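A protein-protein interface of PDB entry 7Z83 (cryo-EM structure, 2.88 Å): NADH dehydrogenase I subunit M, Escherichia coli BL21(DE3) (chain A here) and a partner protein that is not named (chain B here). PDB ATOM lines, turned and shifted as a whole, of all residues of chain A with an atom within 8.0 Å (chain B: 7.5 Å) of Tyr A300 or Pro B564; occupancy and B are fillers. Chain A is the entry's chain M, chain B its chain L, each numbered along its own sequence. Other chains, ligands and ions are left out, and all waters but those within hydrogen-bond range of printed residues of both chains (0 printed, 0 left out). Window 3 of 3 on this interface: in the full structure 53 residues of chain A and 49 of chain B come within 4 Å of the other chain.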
ATOM      1  N   VAL A 238     -14.354 -27.465   0.924  1.00  0.00           N
ATOM      2  CA  VAL A 238     -13.455 -26.500   0.278  1.00  0.00           C
ATOM      3  C   VAL A 238     -12.494 -27.237  -0.645  1.00  0.00           C
ATOM      4  O   VAL A 238     -12.101 -28.383  -0.344  1.00  0.00           O
ATOM      5  CB  VAL A 238     -12.693 -25.684   1.337  1.00  0.00           C
ATOM      6  CG1 VAL A 238     -13.629 -24.697   2.011  1.00  0.00           C
ATOM      7  CG2 VAL A 238     -12.058 -26.601   2.368  1.00  0.00           C
ATOM      8  N   PRO A 239     -12.096 -26.661  -1.793  1.00  0.00           N
ATOM      9  CA  PRO A 239     -12.462 -25.340  -2.316  1.00  0.00           C
ATOM     10  C   PRO A 239     -13.732 -25.357  -3.158  1.00  0.00           C
ATOM     11  O   PRO A 239     -14.068 -24.364  -3.800  1.00  0.00           O
ATOM     12  CB  PRO A 239     -11.258 -24.974  -3.176  1.00  0.00           C
ATOM     13  CG  PRO A 239     -10.792 -26.281  -3.707  1.00  0.00           C
ATOM     14  CD  PRO A 239     -11.137 -27.339  -2.683  1.00  0.00           C
ATOM     15  N   HIS A 241     -16.891 -24.923  -3.022  1.00  0.00           N
ATOM     16  CA  HIS A 241     -17.894 -24.383  -2.111  1.00  0.00           C
ATOM     17  C   HIS A 241     -18.560 -23.087  -2.553  1.00  0.00           C
ATOM     18  O   HIS A 241     -19.593 -22.742  -1.971  1.00  0.00           O
ATOM     19  CB  HIS A 241     -17.276 -24.148  -0.726  1.00  0.00           C
ATOM     20  CG  HIS A 241     -16.255 -23.055  -0.705  1.00  0.00           C
ATOM     21  ND1 HIS A 241     -14.923 -23.277  -0.977  1.00  0.00           N
ATOM     22  CD2 HIS A 241     -16.372 -21.730  -0.455  1.00  0.00           C
ATOM     23  CE1 HIS A 241     -14.262 -22.137  -0.893  1.00  0.00           C
ATOM     24  NE2 HIS A 241     -15.119 -21.183  -0.578  1.00  0.00           N
ATOM     25  N   GLY A 242     -18.024 -22.360  -3.540  1.00  0.00           N
ATOM     26  CA  GLY A 242     -18.514 -21.022  -3.852  1.00  0.00           C
ATOM     27  C   GLY A 242     -19.926 -20.977  -4.402  1.00  0.00           C
ATOM     28  O   GLY A 242     -20.603 -19.940  -4.281  1.00  0.00           O
ATOM     29  N   LEU A 293      -9.449 -31.702   5.362  1.00  0.00           N
ATOM     30  CA  LEU A 293     -10.333 -30.871   4.552  1.00  0.00           C
ATOM     31  C   LEU A 293     -11.492 -30.338   5.380  1.00  0.00           C
ATOM     32  O   LEU A 293     -11.922 -29.199   5.189  1.00  0.00           O
ATOM     33  CB  LEU A 293     -10.855 -31.665   3.356  1.00  0.00           C
ATOM     34  CG  LEU A 293      -9.978 -31.700   2.107  1.00  0.00           C
ATOM     35  CD1 LEU A 293     -10.550 -32.671   1.094  1.00  0.00           C
ATOM     36  CD2 LEU A 293      -9.848 -30.315   1.507  1.00  0.00           C
ATOM     37  N   GLY A 294     -12.007 -31.147   6.307  1.00  0.00           N
ATOM     38  CA  GLY A 294     -13.055 -30.672   7.196  1.00  0.00           C
ATOM     39  C   GLY A 294     -12.580 -29.587   8.145  1.00  0.00           C
ATOM     40  O   GLY A 294     -13.303 -28.623   8.405  1.00  0.00           O
ATOM     41  N   VAL A 295     -11.359 -29.729   8.670  1.00  0.00           N
ATOM     42  CA  VAL A 295     -10.782 -28.695   9.537  1.00  0.00           C
ATOM     43  C   VAL A 295     -10.608 -27.386   8.768  1.00  0.00           C
ATOM     44  O   VAL A 295     -10.994 -26.298   9.236  1.00  0.00           O
ATOM     45  CB  VAL A 295      -9.443 -29.181  10.125  1.00  0.00           C
ATOM     46  CG1 VAL A 295      -8.617 -28.017  10.636  1.00  0.00           C
ATOM     47  CG2 VAL A 295      -9.678 -30.181  11.233  1.00  0.00           C
ATOM     48  N   ILE A 296     -10.032 -27.481   7.564  1.00  0.00           N
ATOM     49  CA  ILE A 296      -9.812 -26.305   6.729  1.00  0.00           C
ATOM     50  C   ILE A 296     -11.144 -25.689   6.322  1.00  0.00           C
ATOM     51  O   ILE A 296     -11.282 -24.465   6.266  1.00  0.00           O
ATOM     52  CB  ILE A 296      -8.942 -26.681   5.513  1.00  0.00           C
ATOM     53  CG1 ILE A 296      -7.515 -26.994   5.964  1.00  0.00           C
ATOM     54  CG2 ILE A 296      -8.910 -25.573   4.473  1.00  0.00           C
ATOM     55  CD1 ILE A 296      -6.665 -27.635   4.893  1.00  0.00           C
ATOM     56  N   GLY A 297     -12.157 -26.524   6.083  1.00  0.00           N
ATOM     57  CA  GLY A 297     -13.476 -26.008   5.766  1.00  0.00           C
ATOM     58  C   GLY A 297     -14.124 -25.284   6.929  1.00  0.00           C
ATOM     59  O   GLY A 297     -14.775 -24.256   6.733  1.00  0.00           O
ATOM     60  N   ILE A 298     -13.944 -25.802   8.150  1.00  0.00           N
ATOM     61  CA  ILE A 298     -14.475 -25.140   9.343  1.00  0.00           C
ATOM     62  C   ILE A 298     -13.879 -23.746   9.485  1.00  0.00           C
ATOM     63  O   ILE A 298     -14.603 -22.749   9.612  1.00  0.00           O
ATOM     64  CB  ILE A 298     -14.203 -25.986  10.600  1.00  0.00           C
ATOM     65  CG1 ILE A 298     -15.145 -27.181  10.671  1.00  0.00           C
ATOM     66  CG2 ILE A 298     -14.360 -25.153  11.862  1.00  0.00           C
ATOM     67  CD1 ILE A 298     -14.826 -28.123  11.797  1.00  0.00           C
ATOM     68  N   PHE A 299     -12.550 -23.650   9.412  1.00  0.00           N
ATOM     69  CA  PHE A 299     -11.936 -22.338   9.612  1.00  0.00           C
ATOM     70  C   PHE A 299     -12.113 -21.412   8.416  1.00  0.00           C
ATOM     71  O   PHE A 299     -12.235 -20.195   8.600  1.00  0.00           O
ATOM     72  CB  PHE A 299     -10.470 -22.493   9.979  1.00  0.00           C
ATOM     73  CG  PHE A 299     -10.276 -22.937  11.381  1.00  0.00           C
ATOM     74  CD1 PHE A 299     -10.479 -22.045  12.418  1.00  0.00           C
ATOM     75  CD2 PHE A 299      -9.958 -24.243  11.675  1.00  0.00           C
ATOM     76  CE1 PHE A 299     -10.325 -22.437  13.722  1.00  0.00           C
ATOM     77  CE2 PHE A 299      -9.814 -24.638  12.977  1.00  0.00           C
ATOM     78  CZ  PHE A 299      -9.987 -23.735  14.002  1.00  0.00           C
ATOM     79  N   TYR A 300     -12.148 -21.953   7.199  1.00  0.00           N
ATOM     80  CA  TYR A 300     -12.420 -21.132   6.029  1.00  0.00           C
ATOM     81  C   TYR A 300     -13.831 -20.567   6.071  1.00  0.00           C
ATOM     82  O   TYR A 300     -14.033 -19.385   5.783  1.00  0.00           O
ATOM     83  CB  TYR A 300     -12.202 -21.950   4.759  1.00  0.00           C
ATOM     84  CG  TYR A 300     -12.024 -21.114   3.517  1.00  0.00           C
ATOM     85  CD1 TYR A 300     -10.770 -20.659   3.137  1.00  0.00           C
ATOM     86  CD2 TYR A 300     -13.112 -20.782   2.723  1.00  0.00           C
ATOM     87  CE1 TYR A 300     -10.606 -19.893   2.002  1.00  0.00           C
ATOM     88  CE2 TYR A 300     -12.957 -20.018   1.589  1.00  0.00           C
ATOM     89  CZ  TYR A 300     -11.704 -19.577   1.232  1.00  0.00           C
ATOM     90  OH  TYR A 300     -11.552 -18.817   0.099  1.00  0.00           O
ATOM     91  N   GLY A 301     -14.816 -21.386   6.450  1.00  0.00           N
ATOM     92  CA  GLY A 301     -16.167 -20.885   6.607  1.00  0.00           C
ATOM     93  C   GLY A 301     -16.296 -19.880   7.730  1.00  0.00           C
ATOM     94  O   GLY A 301     -17.057 -18.919   7.614  1.00  0.00           O
ATOM     95  N   ALA A 302     -15.538 -20.068   8.813  1.00  0.00           N
ATOM     96  CA  ALA A 302     -15.572 -19.107   9.913  1.00  0.00           C
ATOM     97  C   ALA A 302     -15.001 -17.756   9.494  1.00  0.00           C
ATOM     98  O   ALA A 302     -15.633 -16.711   9.703  1.00  0.00           O
ATOM     99  CB  ALA A 302     -14.813 -19.667  11.114  1.00  0.00           C
ATOM    100  N   TRP A 303     -13.809 -17.762   8.891  1.00  0.00           N
ATOM    101  CA  TRP A 303     -13.186 -16.520   8.448  1.00  0.00           C
ATOM    102  C   TRP A 303     -13.963 -15.873   7.310  1.00  0.00           C
ATOM    103  O   TRP A 303     -13.939 -14.646   7.163  1.00  0.00           O
ATOM    104  CB  TRP A 303     -11.745 -16.788   8.022  1.00  0.00           C
ATOM    105  CG  TRP A 303     -10.752 -16.629   9.124  1.00  0.00           C
ATOM    106  CD1 TRP A 303     -10.647 -15.580   9.986  1.00  0.00           C
ATOM    107  CD2 TRP A 303      -9.716 -17.550   9.482  1.00  0.00           C
ATOM    108  NE1 TRP A 303      -9.609 -15.790  10.860  1.00  0.00           N
ATOM    109  CE2 TRP A 303      -9.022 -16.993  10.573  1.00  0.00           C
ATOM    110  CE3 TRP A 303      -9.307 -18.791   8.987  1.00  0.00           C
ATOM    111  CZ2 TRP A 303      -7.939 -17.633  11.174  1.00  0.00           C
ATOM    112  CZ3 TRP A 303      -8.234 -19.425   9.586  1.00  0.00           C
ATOM    113  CH2 TRP A 303      -7.564 -18.846  10.669  1.00  0.00           C
ATOM    114  N   MET A 304     -14.649 -16.677   6.498  1.00  0.00           N
ATOM    115  CA  MET A 304     -15.514 -16.143   5.456  1.00  0.00           C
ATOM    116  C   MET A 304     -16.738 -15.466   6.058  1.00  0.00           C
ATOM    117  O   MET A 304     -17.093 -14.348   5.671  1.00  0.00           O
ATOM    118  CB  MET A 304     -15.933 -17.279   4.521  1.00  0.00           C
ATOM    119  CG  MET A 304     -15.116 -17.553   3.237  1.00  0.00           C
ATOM    120  SD  MET A 304     -14.250 -16.360   2.174  1.00  0.00           S
ATOM    121  CE  MET A 304     -15.229 -14.854   2.190  1.00  0.00           C
ATOM    122  N   ALA A 305     -17.392 -16.131   7.017  1.00  0.00           N
ATOM    123  CA  ALA A 305     -18.622 -15.609   7.600  1.00  0.00           C
ATOM    124  C   ALA A 305     -18.371 -14.373   8.446  1.00  0.00           C
ATOM    125  O   ALA A 305     -19.242 -13.501   8.530  1.00  0.00           O
ATOM    126  CB  ALA A 305     -19.304 -16.688   8.440  1.00  0.00           C
ATOM    127  N   PHE A 306     -17.205 -14.280   9.089  1.00  0.00           N
ATOM    128  CA  PHE A 306     -16.906 -13.074   9.856  1.00  0.00           C
ATOM    129  C   PHE A 306     -16.733 -11.866   8.944  1.00  0.00           C
ATOM    130  O   PHE A 306     -17.125 -10.749   9.301  1.00  0.00           O
ATOM    131  CB  PHE A 306     -15.659 -13.275  10.710  1.00  0.00           C
ATOM    132  CG  PHE A 306     -15.252 -12.046  11.467  1.00  0.00           C
ATOM    133  CD1 PHE A 306     -16.043 -11.564  12.495  1.00  0.00           C
ATOM    134  CD2 PHE A 306     -14.099 -11.358  11.136  1.00  0.00           C
ATOM    135  CE1 PHE A 306     -15.682 -10.428  13.191  1.00  0.00           C
ATOM    136  CE2 PHE A 306     -13.731 -10.222  11.829  1.00  0.00           C
ATOM    137  CZ  PHE A 306     -14.524  -9.757  12.858  1.00  0.00           C
ATOM    138  N   ALA A 307     -16.163 -12.069   7.760  1.00  0.00           N
ATOM    139  CA  ALA A 307     -15.878 -10.984   6.833  1.00  0.00           C
ATOM    140  C   ALA A 307     -17.029 -10.682   5.883  1.00  0.00           C
ATOM    141  O   ALA A 307     -16.878  -9.824   5.008  1.00  0.00           O
ATOM    142  CB  ALA A 307     -14.618 -11.302   6.023  1.00  0.00           C
ATOM    143  N   TYR A 317     -21.829 -19.472   4.838  1.00  0.00           N
ATOM    144  CA  TYR A 317     -20.522 -19.907   5.317  1.00  0.00           C
ATOM    145  C   TYR A 317     -20.607 -20.582   6.685  1.00  0.00           C
ATOM    146  O   TYR A 317     -19.764 -21.431   7.010  1.00  0.00           O
ATOM    147  CB  TYR A 317     -19.562 -18.725   5.328  1.00  0.00           C
ATOM    148  CG  TYR A 317     -19.146 -18.316   3.934  1.00  0.00           C
ATOM    149  CD1 TYR A 317     -18.543 -19.225   3.077  1.00  0.00           C
ATOM    150  CD2 TYR A 317     -19.345 -17.022   3.478  1.00  0.00           C
ATOM    151  CE1 TYR A 317     -18.159 -18.859   1.805  1.00  0.00           C
ATOM    152  CE2 TYR A 317     -18.964 -16.645   2.206  1.00  0.00           C
ATOM    153  CZ  TYR A 317     -18.370 -17.568   1.375  1.00  0.00           C
ATOM    154  OH  TYR A 317     -17.987 -17.197   0.108  1.00  0.00           O
ATOM    155  N   THR A 318     -21.631 -20.246   7.477  1.00  0.00           N
ATOM    156  CA  THR A 318     -21.954 -21.043   8.660  1.00  0.00           C
ATOM    157  C   THR A 318     -22.279 -22.481   8.281  1.00  0.00           C
ATOM    158  O   THR A 318     -21.841 -23.429   8.951  1.00  0.00           O
ATOM    159  CB  THR A 318     -23.138 -20.419   9.397  1.00  0.00           C
ATOM    160  OG1 THR A 318     -23.026 -18.991   9.371  1.00  0.00           O
ATOM    161  CG2 THR A 318     -23.212 -20.916  10.830  1.00  0.00           C
ATOM    162  N   VAL A 320     -21.161 -23.959   5.628  1.00  0.00           N
ATOM    163  CA  VAL A 320     -19.885 -24.534   5.195  1.00  0.00           C
ATOM    164  C   VAL A 320     -19.099 -25.069   6.391  1.00  0.00           C
ATOM    165  O   VAL A 320     -18.589 -26.197   6.369  1.00  0.00           O
ATOM    166  CB  VAL A 320     -19.069 -23.493   4.407  1.00  0.00           C
ATOM    167  CG1 VAL A 320     -17.661 -24.000   4.141  1.00  0.00           C
ATOM    168  CG2 VAL A 320     -19.762 -23.154   3.102  1.00  0.00           C
ATOM    169  N   SER A 321     -19.014 -24.275   7.464  1.00  0.00           N
ATOM    170  CA  SER A 321     -18.263 -24.699   8.647  1.00  0.00           C
ATOM    171  C   SER A 321     -18.912 -25.900   9.339  1.00  0.00           C
ATOM    172  O   SER A 321     -18.220 -26.848   9.740  1.00  0.00           O
ATOM    173  CB  SER A 321     -18.123 -23.532   9.621  1.00  0.00           C
ATOM    174  OG  SER A 321     -19.091 -23.614  10.649  1.00  0.00           O
ATOM    175  N   PHE A 431     -14.410 -20.028  16.985  1.00  0.00           N
ATOM    176  CA  PHE A 431     -14.587 -19.158  15.819  1.00  0.00           C
ATOM    177  C   PHE A 431     -16.062 -19.033  15.431  1.00  0.00           C
ATOM    178  O   PHE A 431     -16.509 -17.972  14.965  1.00  0.00           O
ATOM    179  CB  PHE A 431     -13.778 -19.695  14.638  1.00  0.00           C
ATOM    180  CG  PHE A 431     -12.319 -19.310  14.653  1.00  0.00           C
ATOM    181  CD1 PHE A 431     -11.557 -19.412  15.807  1.00  0.00           C
ATOM    182  CD2 PHE A 431     -11.704 -18.874  13.493  1.00  0.00           C
ATOM    183  CE1 PHE A 431     -10.222 -19.071  15.807  1.00  0.00           C
ATOM    184  CE2 PHE A 431     -10.368 -18.533  13.489  1.00  0.00           C
ATOM    185  CZ  PHE A 431      -9.627 -18.631  14.647  1.00  0.00           C
ATOM    186  N   TYR A 435     -18.158 -15.481  15.021  1.00  0.00           N
ATOM    187  CA  TYR A 435     -18.916 -14.898  13.912  1.00  0.00           C
ATOM    188  C   TYR A 435     -20.403 -14.773  14.226  1.00  0.00           C
ATOM    189  O   TYR A 435     -21.059 -13.871  13.692  1.00  0.00           O
ATOM    190  CB  TYR A 435     -18.688 -15.654  12.588  1.00  0.00           C
ATOM    191  CG  TYR A 435     -19.094 -17.118  12.451  1.00  0.00           C
ATOM    192  CD1 TYR A 435     -20.419 -17.533  12.546  1.00  0.00           C
ATOM    193  CD2 TYR A 435     -18.145 -18.070  12.123  1.00  0.00           C
ATOM    194  CE1 TYR A 435     -20.766 -18.855  12.396  1.00  0.00           C
ATOM    195  CE2 TYR A 435     -18.487 -19.392  11.947  1.00  0.00           C
ATOM    196  CZ  TYR A 435     -19.794 -19.782  12.096  1.00  0.00           C
ATOM    197  OH  TYR A 435     -20.123 -21.107  11.932  1.00  0.00           O
ATOM    198  N   LEU B 559      -7.957 -10.313   4.484  1.00  0.00           N
ATOM    199  CA  LEU B 559      -7.245 -10.940   3.377  1.00  0.00           C
ATOM    200  C   LEU B 559      -8.103 -11.983   2.671  1.00  0.00           C
ATOM    201  O   LEU B 559      -7.905 -12.241   1.479  1.00  0.00           O
ATOM    202  CB  LEU B 559      -5.948 -11.567   3.894  1.00  0.00           C
ATOM    203  CG  LEU B 559      -4.986 -12.230   2.907  1.00  0.00           C
ATOM    204  CD1 LEU B 559      -3.760 -11.361   2.687  1.00  0.00           C
ATOM    205  CD2 LEU B 559      -4.588 -13.610   3.404  1.00  0.00           C
ATOM    206  N   LEU B 560      -9.053 -12.589   3.379  1.00  0.00           N
ATOM    207  CA  LEU B 560      -9.866 -13.661   2.824  1.00  0.00           C
ATOM    208  C   LEU B 560     -11.281 -13.238   2.459  1.00  0.00           C
ATOM    209  O   LEU B 560     -12.052 -14.084   2.003  1.00  0.00           O
ATOM    210  CB  LEU B 560      -9.933 -14.836   3.809  1.00  0.00           C
ATOM    211  CG  LEU B 560      -8.650 -15.632   4.050  1.00  0.00           C
ATOM    212  CD1 LEU B 560      -8.934 -16.834   4.933  1.00  0.00           C
ATOM    213  CD2 LEU B 560      -8.027 -16.066   2.738  1.00  0.00           C
ATOM    214  N   LYS B 561     -11.648 -11.965   2.646  1.00  0.00           N
ATOM    215  CA  LYS B 561     -13.013 -11.531   2.344  1.00  0.00           C
ATOM    216  C   LYS B 561     -13.386 -11.652   0.868  1.00  0.00           C
ATOM    217  O   LYS B 561     -14.579 -11.636   0.546  1.00  0.00           O
ATOM    218  CB  LYS B 561     -13.220 -10.084   2.795  1.00  0.00           C
ATOM    219  CG  LYS B 561     -12.340  -9.073   2.082  1.00  0.00           C
ATOM    220  CD  LYS B 561     -12.926  -7.666   2.140  1.00  0.00           C
ATOM    221  CE  LYS B 561     -13.409  -7.304   3.538  1.00  0.00           C
ATOM    222  NZ  LYS B 561     -14.023  -5.948   3.579  1.00  0.00           N
ATOM    223  N   ARG B 562     -12.415 -11.772  -0.034  1.00  0.00           N
ATOM    224  CA  ARG B 562     -12.707 -11.893  -1.456  1.00  0.00           C
ATOM    225  C   ARG B 562     -12.819 -13.339  -1.929  1.00  0.00           C
ATOM    226  O   ARG B 562     -12.989 -13.563  -3.133  1.00  0.00           O
ATOM    227  CB  ARG B 562     -11.646 -11.160  -2.289  1.00  0.00           C
ATOM    228  CG  ARG B 562     -10.298 -11.862  -2.382  1.00  0.00           C
ATOM    229  CD  ARG B 562      -9.353 -11.403  -1.290  1.00  0.00           C
ATOM    230  NE  ARG B 562      -8.055 -12.060  -1.376  1.00  0.00           N
ATOM    231  CZ  ARG B 562      -6.921 -11.443  -1.681  1.00  0.00           C
ATOM    232  NH1 ARG B 562      -6.888 -10.145  -1.934  1.00  0.00           N
ATOM    233  NH2 ARG B 562      -5.793 -12.146  -1.732  1.00  0.00           N
ATOM    234  N   ASP B 563     -12.734 -14.316  -1.009  1.00  0.00           N
ATOM    235  CA  ASP B 563     -12.866 -15.752  -1.258  1.00  0.00           C
ATOM    236  C   ASP B 563     -11.845 -16.250  -2.279  1.00  0.00           C
ATOM    237  O   ASP B 563     -12.211 -16.514  -3.431  1.00  0.00           O
ATOM    238  CB  ASP B 563     -14.287 -16.092  -1.717  1.00  0.00           C
ATOM    239  CG  ASP B 563     -14.710 -17.492  -1.321  1.00  0.00           C
ATOM    240  OD1 ASP B 563     -13.827 -18.306  -0.983  1.00  0.00           O
ATOM    241  OD2 ASP B 563     -15.925 -17.777  -1.348  1.00  0.00           O
ATOM    242  N   PRO B 564     -10.562 -16.356  -1.908  1.00  0.00           N
ATOM    243  CA  PRO B 564      -9.538 -16.770  -2.886  1.00  0.00           C
ATOM    244  C   PRO B 564      -9.735 -18.163  -3.468  1.00  0.00           C
ATOM    245  O   PRO B 564      -9.378 -18.387  -4.632  1.00  0.00           O
ATOM    246  CB  PRO B 564      -8.233 -16.684  -2.081  1.00  0.00           C
ATOM    247  CG  PRO B 564      -8.541 -15.779  -0.940  1.00  0.00           C
ATOM    248  CD  PRO B 564      -9.968 -16.042  -0.598  1.00  0.00           C
ATOM    249  N   LEU B 565     -10.280 -19.109  -2.696  1.00  0.00           N
ATOM    250  CA  LEU B 565     -10.504 -20.452  -3.226  1.00  0.00           C
ATOM    251  C   LEU B 565     -11.594 -20.462  -4.291  1.00  0.00           C
ATOM    252  O   LEU B 565     -11.527 -21.257  -5.238  1.00  0.00           O
ATOM    253  CB  LEU B 565     -10.857 -21.416  -2.093  1.00  0.00           C
ATOM    254  CG  LEU B 565      -9.771 -21.705  -1.053  1.00  0.00           C
ATOM    255  CD1 LEU B 565     -10.136 -22.928  -0.230  1.00  0.00           C
ATOM    256  CD2 LEU B 565      -8.412 -21.888  -1.707  1.00  0.00           C
ATOM    257  N   ASN B 566     -12.593 -19.587  -4.155  1.00  0.00           N
ATOM    258  CA  ASN B 566     -13.611 -19.448  -5.189  1.00  0.00           C
ATOM    259  C   ASN B 566     -13.004 -18.964  -6.499  1.00  0.00           C
ATOM    260  O   ASN B 566     -13.348 -19.467  -7.574  1.00  0.00           O
ATOM    261  CB  ASN B 566     -14.706 -18.491  -4.717  1.00  0.00           C
ATOM    262  CG  ASN B 566     -15.971 -18.602  -5.536  1.00  0.00           C
ATOM    263  OD1 ASN B 566     -16.118 -19.509  -6.354  1.00  0.00           O
ATOM    264  ND2 ASN B 566     -16.895 -17.676  -5.322  1.00  0.00           N
ATOM    265  N   SER B 567     -12.080 -18.002  -6.429  1.00  0.00           N
ATOM    266  CA  SER B 567     -11.392 -17.544  -7.633  1.00  0.00           C
ATOM    267  C   SER B 567     -10.482 -18.628  -8.201  1.00  0.00           C
ATOM    268  O   SER B 567     -10.363 -18.769  -9.426  1.00  0.00           O
ATOM    269  CB  SER B 567     -10.595 -16.277  -7.328  1.00  0.00           C
ATOM    270  OG  SER B 567     -11.422 -15.285  -6.745  1.00  0.00           O
ATOM    271  N   MET B 568      -9.836 -19.402  -7.321  1.00  0.00           N
ATOM    272  CA  MET B 568      -8.983 -20.499  -7.766  1.00  0.00           C
ATOM    273  C   MET B 568      -9.782 -21.542  -8.538  1.00  0.00           C
ATOM    274  O   MET B 568      -9.332 -22.037  -9.578  1.00  0.00           O
ATOM    275  CB  MET B 568      -8.284 -21.135  -6.561  1.00  0.00           C
ATOM    276  CG  MET B 568      -7.798 -22.559  -6.784  1.00  0.00           C
ATOM    277  SD  MET B 568      -7.800 -23.549  -5.278  1.00  0.00           S
ATOM    278  CE  MET B 568      -6.149 -23.232  -4.665  1.00  0.00           C
ATOM    279  N   MET B 569     -10.979 -21.868  -8.059  1.00  0.00           N
ATOM    280  CA  MET B 569     -11.830 -22.808  -8.776  1.00  0.00           C
ATOM    281  C   MET B 569     -12.590 -22.172  -9.937  1.00  0.00           C
ATOM    282  O   MET B 569     -13.125 -22.905 -10.774  1.00  0.00           O
ATOM    283  CB  MET B 569     -12.812 -23.468  -7.809  1.00  0.00           C
ATOM    284  CG  MET B 569     -12.174 -24.476  -6.872  1.00  0.00           C
ATOM    285  SD  MET B 569     -11.161 -25.691  -7.737  1.00  0.00           S
ATOM    286  CE  MET B 569     -12.377 -26.483  -8.788  1.00  0.00           C
ATOM    287  N   ASN B 570     -12.665 -20.843 -10.004  1.00  0.00           N
ATOM    288  CA  ASN B 570     -13.249 -20.163 -11.153  1.00  0.00           C
ATOM    289  C   ASN B 570     -12.245 -19.904 -12.267  1.00  0.00           C
ATOM    290  O   ASN B 570     -12.652 -19.492 -13.358  1.00  0.00           O
ATOM    291  CB  ASN B 570     -13.874 -18.832 -10.723  1.00  0.00           C
ATOM    292  CG  ASN B 570     -15.293 -18.991 -10.220  1.00  0.00           C
ATOM    293  OD1 ASN B 570     -15.804 -20.105 -10.114  1.00  0.00           O
ATOM    294  ND2 ASN B 570     -15.940 -17.874  -9.911  1.00  0.00           N
ATOM    295  N   ILE B 571     -10.957 -20.097 -11.999  1.00  0.00           N
ATOM    296  CA  ILE B 571      -9.894 -20.021 -13.007  1.00  0.00           C
ATOM    297  C   ILE B 571     -10.153 -20.911 -14.231  1.00  0.00           C
ATOM    298  O   ILE B 571      -9.945 -20.428 -15.359  1.00  0.00           O
ATOM    299  CB  ILE B 571      -8.523 -20.313 -12.357  1.00  0.00           C
ATOM    300  CG1 ILE B 571      -7.976 -19.069 -11.647  1.00  0.00           C
ATOM    301  CG2 ILE B 571      -7.503 -20.845 -13.362  1.00  0.00           C
ATOM    302  CD1 ILE B 571      -8.201 -17.761 -12.387  1.00  0.00           C
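A ring nitrogen (NE2) of His A241 lies within hydrogen-bond range of the side-chain carboxylate of Asp B563.
The side-chain hydroxyl of Tyr A300 lies within hydrogen-bond range of the side-chain carboxylate of Asp B563, 2.6 Å away.
The side-chain hydroxyl (OH) of Tyr A300 sits at hydrogen-bond distance from the backbone NH (N) of Leu B565 (3.1 Å).
The side-chain carboxylate of Asp B563 lies within hydrogen-bond range of the side-chain hydroxyl of Tyr A317 (2.6 Å).
The side-chain hydroxyl (OH) of Tyr A300 lies close to the backbone nitrogen (N) of Pro B564, 3.3 Å away.
The side-chain sulfur of Met A304 sits close to the backbone carbonyl oxygen of Leu B560 (3.2 Å).
SD of Met A304 lies close to OD1 of Asp B563, at 3.7 Å.
O of Pro A239 is in hydrogen-bond range of ND1 of His A241, at 3.1 Å.
Among the printed residues, pairs that only touch across the chains: Pro A239 with Met B569 (3.6 Å), Met A304 with Lys B561 (3.7 Å), His A241 with Leu B565 (3.7 Å), Ala A307 with Lys B561 (3.7 Å), Pro A239 with Leu B565 (3.7 Å) and Gly A242 with Asn B566 (3.8 Å).
Of chain B, only Asp B563, Pro B564 and Leu B565 come within 4 Å of Tyr A300.
Pro B564 touches just one residue of chain A: Tyr A300 (3.3 Å).
Printed residues of chain B within 4 Å of His A241: Asp B563 and Leu B565.
Printed residues of chain A within 4 Å of Asn B566: Gly A242.
Of the printed residues of chain A, Asp B563 touches His A241 (3.2 Å), Tyr A300 (2.6 Å), Met A304 (3.7 Å) and Tyr A317 (2.6 Å).
Ile A298 touches none of the printed residues of chain B.
Val A295 touches none of the printed residues of chain B.
The nearest residue of chain A that does not touch Pro B564 is Met A304 (5.1 Å).
Of the 13 printed residues of chain B, 7 touch a printed residue of chain A.
Hydrophobic or aromatic side chains of chain A within 4 Å of the printed part of chain B: Pro A239, His A241, Tyr A300, Met A304, Ala A307 and Tyr A317.
Among the printed residues, no Asp or Glu carboxylate lies within 4 Å of a Lys or Arg side-chain nitrogen of the other chain.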
